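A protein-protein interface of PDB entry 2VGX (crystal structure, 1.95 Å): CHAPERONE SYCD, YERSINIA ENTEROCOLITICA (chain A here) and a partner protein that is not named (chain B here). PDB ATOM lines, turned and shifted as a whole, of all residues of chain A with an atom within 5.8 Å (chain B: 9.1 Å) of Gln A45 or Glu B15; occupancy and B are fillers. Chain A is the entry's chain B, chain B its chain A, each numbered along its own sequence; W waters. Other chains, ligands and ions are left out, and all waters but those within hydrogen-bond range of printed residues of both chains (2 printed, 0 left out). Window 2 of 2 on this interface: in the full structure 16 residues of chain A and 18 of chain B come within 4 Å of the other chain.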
ATOM      1  N   ALA A  40       9.788   1.710  11.745  1.00  0.00           N
ATOM      2  CA  ALA A  40       8.774   1.275  10.769  1.00  0.00           C
ATOM      3  C   ALA A  40       8.189   2.499  10.066  1.00  0.00           C
ATOM      4  O   ALA A  40       7.915   2.462   8.872  1.00  0.00           O
ATOM      5  CB  ALA A  40       7.651   0.489  11.476  1.00  0.00           C
ATOM      6  N   HIS A  41       8.011   3.575  10.829  1.00  0.00           N
ATOM      7  CA  HIS A  41       7.455   4.839  10.336  1.00  0.00           C
ATOM      8  C   HIS A  41       8.304   5.441   9.219  1.00  0.00           C
ATOM      9  O   HIS A  41       7.753   5.918   8.198  1.00  0.00           O
ATOM     10  CB  HIS A  41       7.314   5.859  11.478  1.00  0.00           C
ATOM     11  CG  HIS A  41       6.663   7.149  11.061  1.00  0.00           C
ATOM     12  ND1 HIS A  41       7.314   8.117  10.322  1.00  0.00           N
ATOM     13  CD2 HIS A  41       5.403   7.616  11.255  1.00  0.00           C
ATOM     14  CE1 HIS A  41       6.494   9.134  10.101  1.00  0.00           C
ATOM     15  NE2 HIS A  41       5.330   8.856  10.665  1.00  0.00           N
ATOM     16  N   MLY A  42       9.622   5.409   9.396  1.00  0.00           N
ATOM     17  CA  MLY A  42      10.585   5.912   8.357  1.00  0.00           C
ATOM     18  CB  MLY A  42      12.055   5.765   8.801  1.00  0.00           C
ATOM     19  CG  MLY A  42      12.338   6.737   9.945  1.00  0.00           C
ATOM     20  CD  MLY A  42      13.711   6.423  10.544  1.00  0.00           C
ATOM     21  CE  MLY A  42      13.916   7.359  11.754  1.00  0.00           C
ATOM     22  NZ  MLY A  42      15.349   7.354  12.008  1.00  0.00           N
ATOM     23  CH1 MLY A  42      16.213   8.229  11.211  1.00  0.00           C
ATOM     24  CH2 MLY A  42      15.874   6.447  13.023  1.00  0.00           C
ATOM     25  C   MLY A  42      10.422   5.185   7.059  1.00  0.00           C
ATOM     26  O   MLY A  42      10.310   5.813   6.015  1.00  0.00           O
ATOM     27  N   VAL A  43      10.391   3.863   7.123  1.00  0.00           N
ATOM     28  CA  VAL A  43      10.213   3.024   5.954  1.00  0.00           C
ATOM     29  C   VAL A  43       8.834   3.215   5.289  1.00  0.00           C
ATOM     30  O   VAL A  43       8.789   3.420   4.078  1.00  0.00           O
ATOM     31  CB  VAL A  43      10.476   1.560   6.215  1.00  0.00           C
ATOM     32  CG1 VAL A  43      10.336   0.773   4.892  1.00  0.00           C
ATOM     33  CG2 VAL A  43      11.906   1.351   6.843  1.00  0.00           C
ATOM     34  N   PHE A  44       7.744   3.155   6.064  1.00  0.00           N
ATOM     35  CA  PHE A  44       6.402   3.400   5.517  1.00  0.00           C
ATOM     36  C   PHE A  44       6.268   4.768   4.906  1.00  0.00           C
ATOM     37  O   PHE A  44       5.641   4.923   3.872  1.00  0.00           O
ATOM     38  CB  PHE A  44       5.309   3.240   6.591  1.00  0.00           C
ATOM     39  CG  PHE A  44       4.943   1.809   6.852  1.00  0.00           C
ATOM     40  CD1 PHE A  44       4.548   0.988   5.791  1.00  0.00           C
ATOM     41  CD2 PHE A  44       4.949   1.291   8.154  1.00  0.00           C
ATOM     42  CE1 PHE A  44       4.209  -0.334   6.009  1.00  0.00           C
ATOM     43  CE2 PHE A  44       4.604  -0.049   8.387  1.00  0.00           C
ATOM     44  CZ  PHE A  44       4.233  -0.852   7.325  1.00  0.00           C
ATOM     45  N   GLN A  45       6.800   5.786   5.572  1.00  0.00           N
ATOM     46  CA  GLN A  45       6.783   7.118   4.982  1.00  0.00           C
ATOM     47  C   GLN A  45       7.479   7.167   3.594  1.00  0.00           C
ATOM     48  O   GLN A  45       6.951   7.789   2.646  1.00  0.00           O
ATOM     49  CB  GLN A  45       7.432   8.117   5.909  1.00  0.00           C
ATOM     50  CG  GLN A  45       7.346   9.500   5.376  1.00  0.00           C
ATOM     51  CD  GLN A  45       7.867  10.517   6.357  1.00  0.00           C
ATOM     52  OE1 GLN A  45       8.879  10.287   7.033  1.00  0.00           O
ATOM     53  NE2 GLN A  45       7.185  11.650   6.441  1.00  0.00           N
ATOM     54  N   ALA A  46       8.653   6.543   3.463  1.00  0.00           N
ATOM     55  CA  ALA A  46       9.337   6.466   2.150  1.00  0.00           C
ATOM     56  C   ALA A  46       8.483   5.704   1.134  1.00  0.00           C
ATOM     57  O   ALA A  46       8.411   6.083  -0.033  1.00  0.00           O
ATOM     58  CB  ALA A  46      10.729   5.774   2.282  1.00  0.00           C
ATOM     59  N   LEU A  47       7.803   4.654   1.593  1.00  0.00           N
ATOM     60  CA  LEU A  47       6.959   3.834   0.715  1.00  0.00           C
ATOM     61  C   LEU A  47       5.770   4.661   0.191  1.00  0.00           C
ATOM     62  O   LEU A  47       5.427   4.577  -0.994  1.00  0.00           O
ATOM     63  CB  LEU A  47       6.472   2.569   1.443  1.00  0.00           C
ATOM     64  CG  LEU A  47       7.530   1.458   1.682  1.00  0.00           C
ATOM     65  CD1 LEU A  47       7.004   0.358   2.619  1.00  0.00           C
ATOM     66  CD2 LEU A  47       7.956   0.875   0.329  1.00  0.00           C
ATOM     67  N   CYS A  48       5.170   5.464   1.076  1.00  0.00           N
ATOM     68  CA  CYS A  48       4.025   6.317   0.707  1.00  0.00           C
ATOM     69  C   CYS A  48       4.434   7.325  -0.364  1.00  0.00           C
ATOM     70  O   CYS A  48       3.635   7.651  -1.246  1.00  0.00           O
ATOM     71  CB  CYS A  48       3.489   7.058   1.911  1.00  0.00           C
ATOM     72  SG  CYS A  48       2.541   6.003   3.059  1.00  0.00           S
ATOM     73  N   VAL A  49       5.664   7.814  -0.282  1.00  0.00           N
ATOM     74  CA  VAL A  49       6.209   8.726  -1.306  1.00  0.00           C
ATOM     75  C   VAL A  49       6.454   8.058  -2.654  1.00  0.00           C
ATOM     76  O   VAL A  49       6.167   8.658  -3.739  1.00  0.00           O
ATOM     77  CB  VAL A  49       7.459   9.441  -0.766  1.00  0.00           C
ATOM     78  CG1 VAL A  49       8.144  10.298  -1.841  1.00  0.00           C
ATOM     79  CG2 VAL A  49       7.048  10.318   0.438  1.00  0.00           C
ATOM     80  N   LEU A  50       6.980   6.828  -2.588  1.00  0.00           N
ATOM     81  CA  LEU A  50       7.294   6.043  -3.783  1.00  0.00           C
ATOM     82  C   LEU A  50       6.064   5.550  -4.513  1.00  0.00           C
ATOM     83  O   LEU A  50       6.074   5.489  -5.742  1.00  0.00           O
ATOM     84  CB  LEU A  50       8.270   4.902  -3.457  1.00  0.00           C
ATOM     85  CG  LEU A  50       9.692   5.332  -3.030  1.00  0.00           C
ATOM     86  CD1 LEU A  50      10.385   4.294  -2.083  1.00  0.00           C
ATOM     87  CD2 LEU A  50      10.573   5.697  -4.245  1.00  0.00           C
ATOM     88  N   LEU A  61       1.592   3.462   7.798  1.00  0.00           N
ATOM     89  CA  LEU A  61       2.053   4.778   8.283  1.00  0.00           C
ATOM     90  C   LEU A  61       1.135   5.268   9.389  1.00  0.00           C
ATOM     91  O   LEU A  61       1.590   5.831  10.427  1.00  0.00           O
ATOM     92  CB  LEU A  61       2.076   5.804   7.127  1.00  0.00           C
ATOM     93  CG  LEU A  61       2.609   7.196   7.511  1.00  0.00           C
ATOM     94  CD1 LEU A  61       4.129   7.038   7.761  1.00  0.00           C
ATOM     95  CD2 LEU A  61       2.316   8.180   6.422  1.00  0.00           C
ATOM     96  N   ARG A  65       1.967   5.850  13.462  1.00  0.00           N
ATOM     97  CA  ARG A  65       1.693   7.130  14.104  1.00  0.00           C
ATOM     98  C   ARG A  65       0.763   6.928  15.295  1.00  0.00           C
ATOM     99  O   ARG A  65       0.980   7.527  16.362  1.00  0.00           O
ATOM    100  CB  ARG A  65       1.087   8.126  13.106  1.00  0.00           C
ATOM    101  CG  ARG A  65       2.089   8.623  12.076  1.00  0.00           C
ATOM    102  CD  ARG A  65       1.439   9.264  10.849  1.00  0.00           C
ATOM    103  NE  ARG A  65       2.503   9.936  10.114  1.00  0.00           N
ATOM    104  CZ  ARG A  65       2.336  10.768   9.095  1.00  0.00           C
ATOM    105  NH1 ARG A  65       1.106  11.047   8.674  1.00  0.00           N
ATOM    106  NH2 ARG A  65       3.423  11.333   8.515  1.00  0.00           N
ATOM    107  N   THR B   9      14.681  18.045  -4.105  1.00  0.00           N
ATOM    108  CA  THR B   9      14.511  16.603  -4.258  1.00  0.00           C
ATOM    109  C   THR B   9      13.110  16.176  -3.815  1.00  0.00           C
ATOM    110  O   THR B   9      12.431  16.877  -3.082  1.00  0.00           O
ATOM    111  CB  THR B   9      15.549  15.793  -3.417  1.00  0.00           C
ATOM    112  OG1 THR B   9      15.316  16.026  -2.013  1.00  0.00           O
ATOM    113  CG2 THR B   9      16.978  16.147  -3.785  1.00  0.00           C
ATOM    114  N   ILE B  10      12.688  15.002  -4.253  1.00  0.00           N
ATOM    115  CA  ILE B  10      11.423  14.429  -3.829  1.00  0.00           C
ATOM    116  C   ILE B  10      11.395  14.188  -2.322  1.00  0.00           C
ATOM    117  O   ILE B  10      10.387  14.440  -1.677  1.00  0.00           O
ATOM    118  CB  ILE B  10      11.171  13.049  -4.560  1.00  0.00           C
ATOM    119  CG1 ILE B  10      11.060  13.214  -6.096  1.00  0.00           C
ATOM    120  CG2 ILE B  10       9.952  12.313  -3.985  1.00  0.00           C
ATOM    121  CD1 ILE B  10      10.043  14.229  -6.565  1.00  0.00           C
ATOM    122  N   ALA B  11      12.478  13.654  -1.764  1.00  0.00           N
ATOM    123  CA  ALA B  11      12.538  13.428  -0.332  1.00  0.00           C
ATOM    124  C   ALA B  11      12.372  14.743   0.424  1.00  0.00           C
ATOM    125  O   ALA B  11      11.618  14.781   1.368  1.00  0.00           O
ATOM    126  CB  ALA B  11      13.860  12.729   0.098  1.00  0.00           C
ATOM    127  N   MET B  12      13.062  15.800   0.001  1.00  0.00           N
ATOM    128  CA  MET B  12      12.964  17.116   0.690  1.00  0.00           C
ATOM    129  C   MET B  12      11.534  17.642   0.649  1.00  0.00           C
ATOM    130  O   MET B  12      10.992  18.056   1.671  1.00  0.00           O
ATOM    131  CB  MET B  12      13.866  18.161   0.055  1.00  0.00           C
ATOM    132  CG  MET B  12      15.333  17.981   0.300  1.00  0.00           C
ATOM    133  SD  MET B  12      16.262  19.076  -0.785  1.00  0.00           S
ATOM    134  CE  MET B  12      15.758  20.637  -0.003  1.00  0.00           C
ATOM    135  N   LEU B  13      10.907  17.596  -0.525  1.00  0.00           N
ATOM    136  CA  LEU B  13       9.534  18.047  -0.668  1.00  0.00           C
ATOM    137  C   LEU B  13       8.638  17.298   0.294  1.00  0.00           C
ATOM    138  O   LEU B  13       7.745  17.884   0.919  1.00  0.00           O
ATOM    139  CB  LEU B  13       9.028  17.849  -2.102  1.00  0.00           C
ATOM    140  CG  LEU B  13       9.357  18.912  -3.144  1.00  0.00           C
ATOM    141  CD1 LEU B  13       9.053  18.346  -4.536  1.00  0.00           C
ATOM    142  CD2 LEU B  13       8.568  20.201  -2.894  1.00  0.00           C
ATOM    143  N   ASN B  14       8.893  16.001   0.450  1.00  0.00           N
ATOM    144  CA  ASN B  14       8.024  15.178   1.280  1.00  0.00           C
ATOM    145  C   ASN B  14       8.412  15.029   2.745  1.00  0.00           C
ATOM    146  O   ASN B  14       7.841  14.204   3.472  1.00  0.00           O
ATOM    147  CB  ASN B  14       7.883  13.816   0.622  1.00  0.00           C
ATOM    148  CG  ASN B  14       7.023  13.877  -0.590  1.00  0.00           C
ATOM    149  OD1 ASN B  14       5.805  13.786  -0.471  1.00  0.00           O
ATOM    150  ND2 ASN B  14       7.640  14.047  -1.780  1.00  0.00           N
ATOM    151  N   GLU B  15       9.375  15.835   3.168  1.00  0.00           N
ATOM    152  CA  GLU B  15       9.888  15.841   4.536  1.00  0.00           C
ATOM    153  C   GLU B  15      10.451  14.486   4.969  1.00  0.00           C
ATOM    154  O   GLU B  15      10.254  14.056   6.104  1.00  0.00           O
ATOM    155  CB  GLU B  15       8.809  16.369   5.499  1.00  0.00           C
ATOM    156  CG  GLU B  15       8.372  17.801   5.131  1.00  0.00           C
ATOM    157  CD  GLU B  15       7.154  18.282   5.913  1.00  0.00           C
ATOM    158  OE1 GLU B  15       6.326  17.444   6.371  1.00  0.00           O
ATOM    159  OE2 GLU B  15       7.028  19.526   6.054  1.00  0.00           O
ATOM    160  N   ILE B  16      11.124  13.809   4.035  1.00  0.00           N
ATOM    161  CA  ILE B  16      11.885  12.611   4.360  1.00  0.00           C
ATOM    162  C   ILE B  16      13.296  13.122   4.646  1.00  0.00           C
ATOM    163  O   ILE B  16      13.919  13.757   3.784  1.00  0.00           O
ATOM    164  CB  ILE B  16      11.912  11.623   3.189  1.00  0.00           C
ATOM    165  CG1 ILE B  16      10.491  11.034   3.012  1.00  0.00           C
ATOM    166  CG2 ILE B  16      12.885  10.483   3.465  1.00  0.00           C
ATOM    167  CD1 ILE B  16      10.375  10.169   1.811  1.00  0.00           C
ATOM    168  N   SER B  17      13.777  12.864   5.858  1.00  0.00           N
ATOM    169  CA  SER B  17      15.048  13.411   6.290  1.00  0.00           C
ATOM    170  C   SER B  17      16.188  12.576   5.702  1.00  0.00           C
ATOM    171  O   SER B  17      16.026  11.371   5.394  1.00  0.00           O
ATOM    172  CB  SER B  17      15.136  13.409   7.817  1.00  0.00           C
ATOM    173  OG  SER B  17      15.092  12.086   8.303  1.00  0.00           O
ATOM    174  N   SER B  18      17.334  13.215   5.566  1.00  0.00           N
ATOM    175  CA  SER B  18      18.506  12.539   5.028  1.00  0.00           C
ATOM    176  C   SER B  18      18.993  11.388   5.906  1.00  0.00           C
ATOM    177  O   SER B  18      19.676  10.511   5.401  1.00  0.00           O
ATOM    178  CB  SER B  18      19.612  13.542   4.728  1.00  0.00           C
ATOM    179  OG  SER B  18      19.229  14.318   3.611  1.00  0.00           O
ATOM    180  N   ASP B  19      18.618  11.400   7.189  1.00  0.00           N
ATOM    181  CA  ASP B  19      18.819  10.286   8.147  1.00  0.00           C
ATOM    182  C   ASP B  19      18.014   9.015   7.819  1.00  0.00           C
ATOM    183  O   ASP B  19      18.468   7.889   8.103  1.00  0.00           O
ATOM    184  CB  ASP B  19      18.373  10.688   9.561  1.00  0.00           C
ATOM    185  CG  ASP B  19      19.104  11.897  10.112  1.00  0.00           C
ATOM    186  OD1 ASP B  19      20.318  11.776  10.420  1.00  0.00           O
ATOM    187  OD2 ASP B  19      18.449  12.969  10.266  1.00  0.00           O
ATOM    188  N   THR B  20      16.788   9.186   7.308  1.00  0.00           N
ATOM    189  CA  THR B  20      16.029   8.056   6.744  1.00  0.00           C
ATOM    190  C   THR B  20      16.712   7.523   5.480  1.00  0.00           C
ATOM    191  O   THR B  20      16.835   6.303   5.293  1.00  0.00           O
ATOM    192  CB  THR B  20      14.574   8.440   6.428  1.00  0.00           C
ATOM    193  OG1 THR B  20      13.885   8.640   7.662  1.00  0.00           O
ATOM    194  CG2 THR B  20      13.830   7.346   5.619  1.00  0.00           C
ATOM    195  N   LEU B  21      17.182   8.431   4.624  1.00  0.00           N
ATOM    196  CA  LEU B  21      17.863   8.020   3.404  1.00  0.00           C
ATOM    197  C   LEU B  21      19.125   7.263   3.714  1.00  0.00           C
ATOM    198  O   LEU B  21      19.438   6.275   3.049  1.00  0.00           O
ATOM    199  CB  LEU B  21      18.154   9.239   2.537  1.00  0.00           C
ATOM    200  CG  LEU B  21      16.890   9.974   2.061  1.00  0.00           C
ATOM    201  CD1 LEU B  21      17.284  11.183   1.239  1.00  0.00           C
ATOM    202  CD2 LEU B  21      15.944   9.109   1.267  1.00  0.00           C
ATOM    203  N   LEU B  24      18.351   3.678   4.696  1.00  0.00           N
ATOM    204  CA  LEU B  24      18.060   2.908   3.487  1.00  0.00           C
ATOM    205  C   LEU B  24      19.306   2.648   2.670  1.00  0.00           C
ATOM    206  O   LEU B  24      19.457   1.570   2.077  1.00  0.00           O
ATOM    207  CB  LEU B  24      17.057   3.674   2.611  1.00  0.00           C
ATOM    208  CG  LEU B  24      15.669   3.825   3.171  1.00  0.00           C
ATOM    209  CD1 LEU B  24      14.836   4.759   2.270  1.00  0.00           C
ATOM    210  CD2 LEU B  24      15.029   2.433   3.247  1.00  0.00           C
ATOM    211  N   LEU B  50      14.304   9.348  -4.705  1.00  0.00           N
ATOM    212  CA  LEU B  50      14.157  10.164  -3.460  1.00  0.00           C
ATOM    213  C   LEU B  50      15.136  11.308  -3.397  1.00  0.00           C
ATOM    214  O   LEU B  50      14.756  12.394  -2.939  1.00  0.00           O
ATOM    215  CB  LEU B  50      14.240   9.310  -2.173  1.00  0.00           C
ATOM    216  CG  LEU B  50      12.994   8.389  -2.009  1.00  0.00           C
ATOM    217  CD1 LEU B  50      13.176   7.359  -0.892  1.00  0.00           C
ATOM    218  CD2 LEU B  50      11.679   9.140  -1.786  1.00  0.00           C
HETATM  219  O   HOH W   1       5.600  12.625   4.308  1.00  0.00           O
HETATM  220  O   HOH W   2      10.716   8.631   6.273  1.00  0.00           O
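Of the 15 printed residues of chain B, 7 touch a printed residue of chain A. Printed residues of chain B that touch a printed residue of chain A: Ile B10, Asn B14, Glu B15, Ile B16, Asp B19, Thr B20 and Leu B50. Hydrophobic or aromatic side chains of chain B that line the printed part of chain A: Ile B10, Ile B16 and Leu B50. Hydrophobic or aromatic side chains of chain A that line the printed part of chain B: Val A49. Among the printed residues, no Asp or Glu carboxylate lies within 4 Å of a Lys or Arg side-chain nitrogen of the other chain.
Gln A45 touches just these residues of chain B: Asn B14 (3.97 Å) and Glu B15 (3.9 Å). Ala A46 touches just one residue of chain B: Ile B16. Of the printed residues of chain A, Ile B10 touches Val A49. Printed residues of chain A within 4 Å of Asn B14: Gln A45 (3.97 Å) and Val A49 (3.6 Å). Glu B15 touches just one residue of chain A: Gln A45 (3.9 Å). The nearest printed residue of chain A that does not touch Glu B15 is Val A49 (6.6 Å).
Water W2 lies within hydrogen-bond range of the side-chain amide oxygen (OE1) of Gln A45 (2.6 Å), O of MLY A42 (2.9 Å) and the side-chain hydroxyl (OG1) of Thr B20 (3.5 Å). Water W1 bridges the side-chain amide nitrogen of Gln A45 (2.8 Å) and the backbone carbonyl oxygen of Asn B14 (2.9 Å).
Asp B19 touches MLY A42. Thr B20 touches MLY A42 (OG1 to CG, 3.4 Å). Asn B14 touches Gln A45 (O to NE2, 3.97 Å). Gln A45 touches Glu B15. Ile B16 touches Ala A46. Val A49 touches Ile B10 (CG1 to CG2, 3.5 Å). CG2 of Val A49 touches CB of Asn B14, at 3.6 Å. Ile B16 touches Val A49 (CD1 to CG2, 3.6 Å). Val A49 touches Leu B50.
The backbone carbonyl oxygen of Ile B10 is in hydrogen-bond range of the side-chain amide nitrogen of Asn B14. O of Ala B11 sits at hydrogen-bond distance from N of Ile B16 (2.9 Å). The backbone carbonyl oxygen (O) of Leu B50 lies within hydrogen-bond range of the backbone NH (N) of Ala B11 (2.9 Å).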
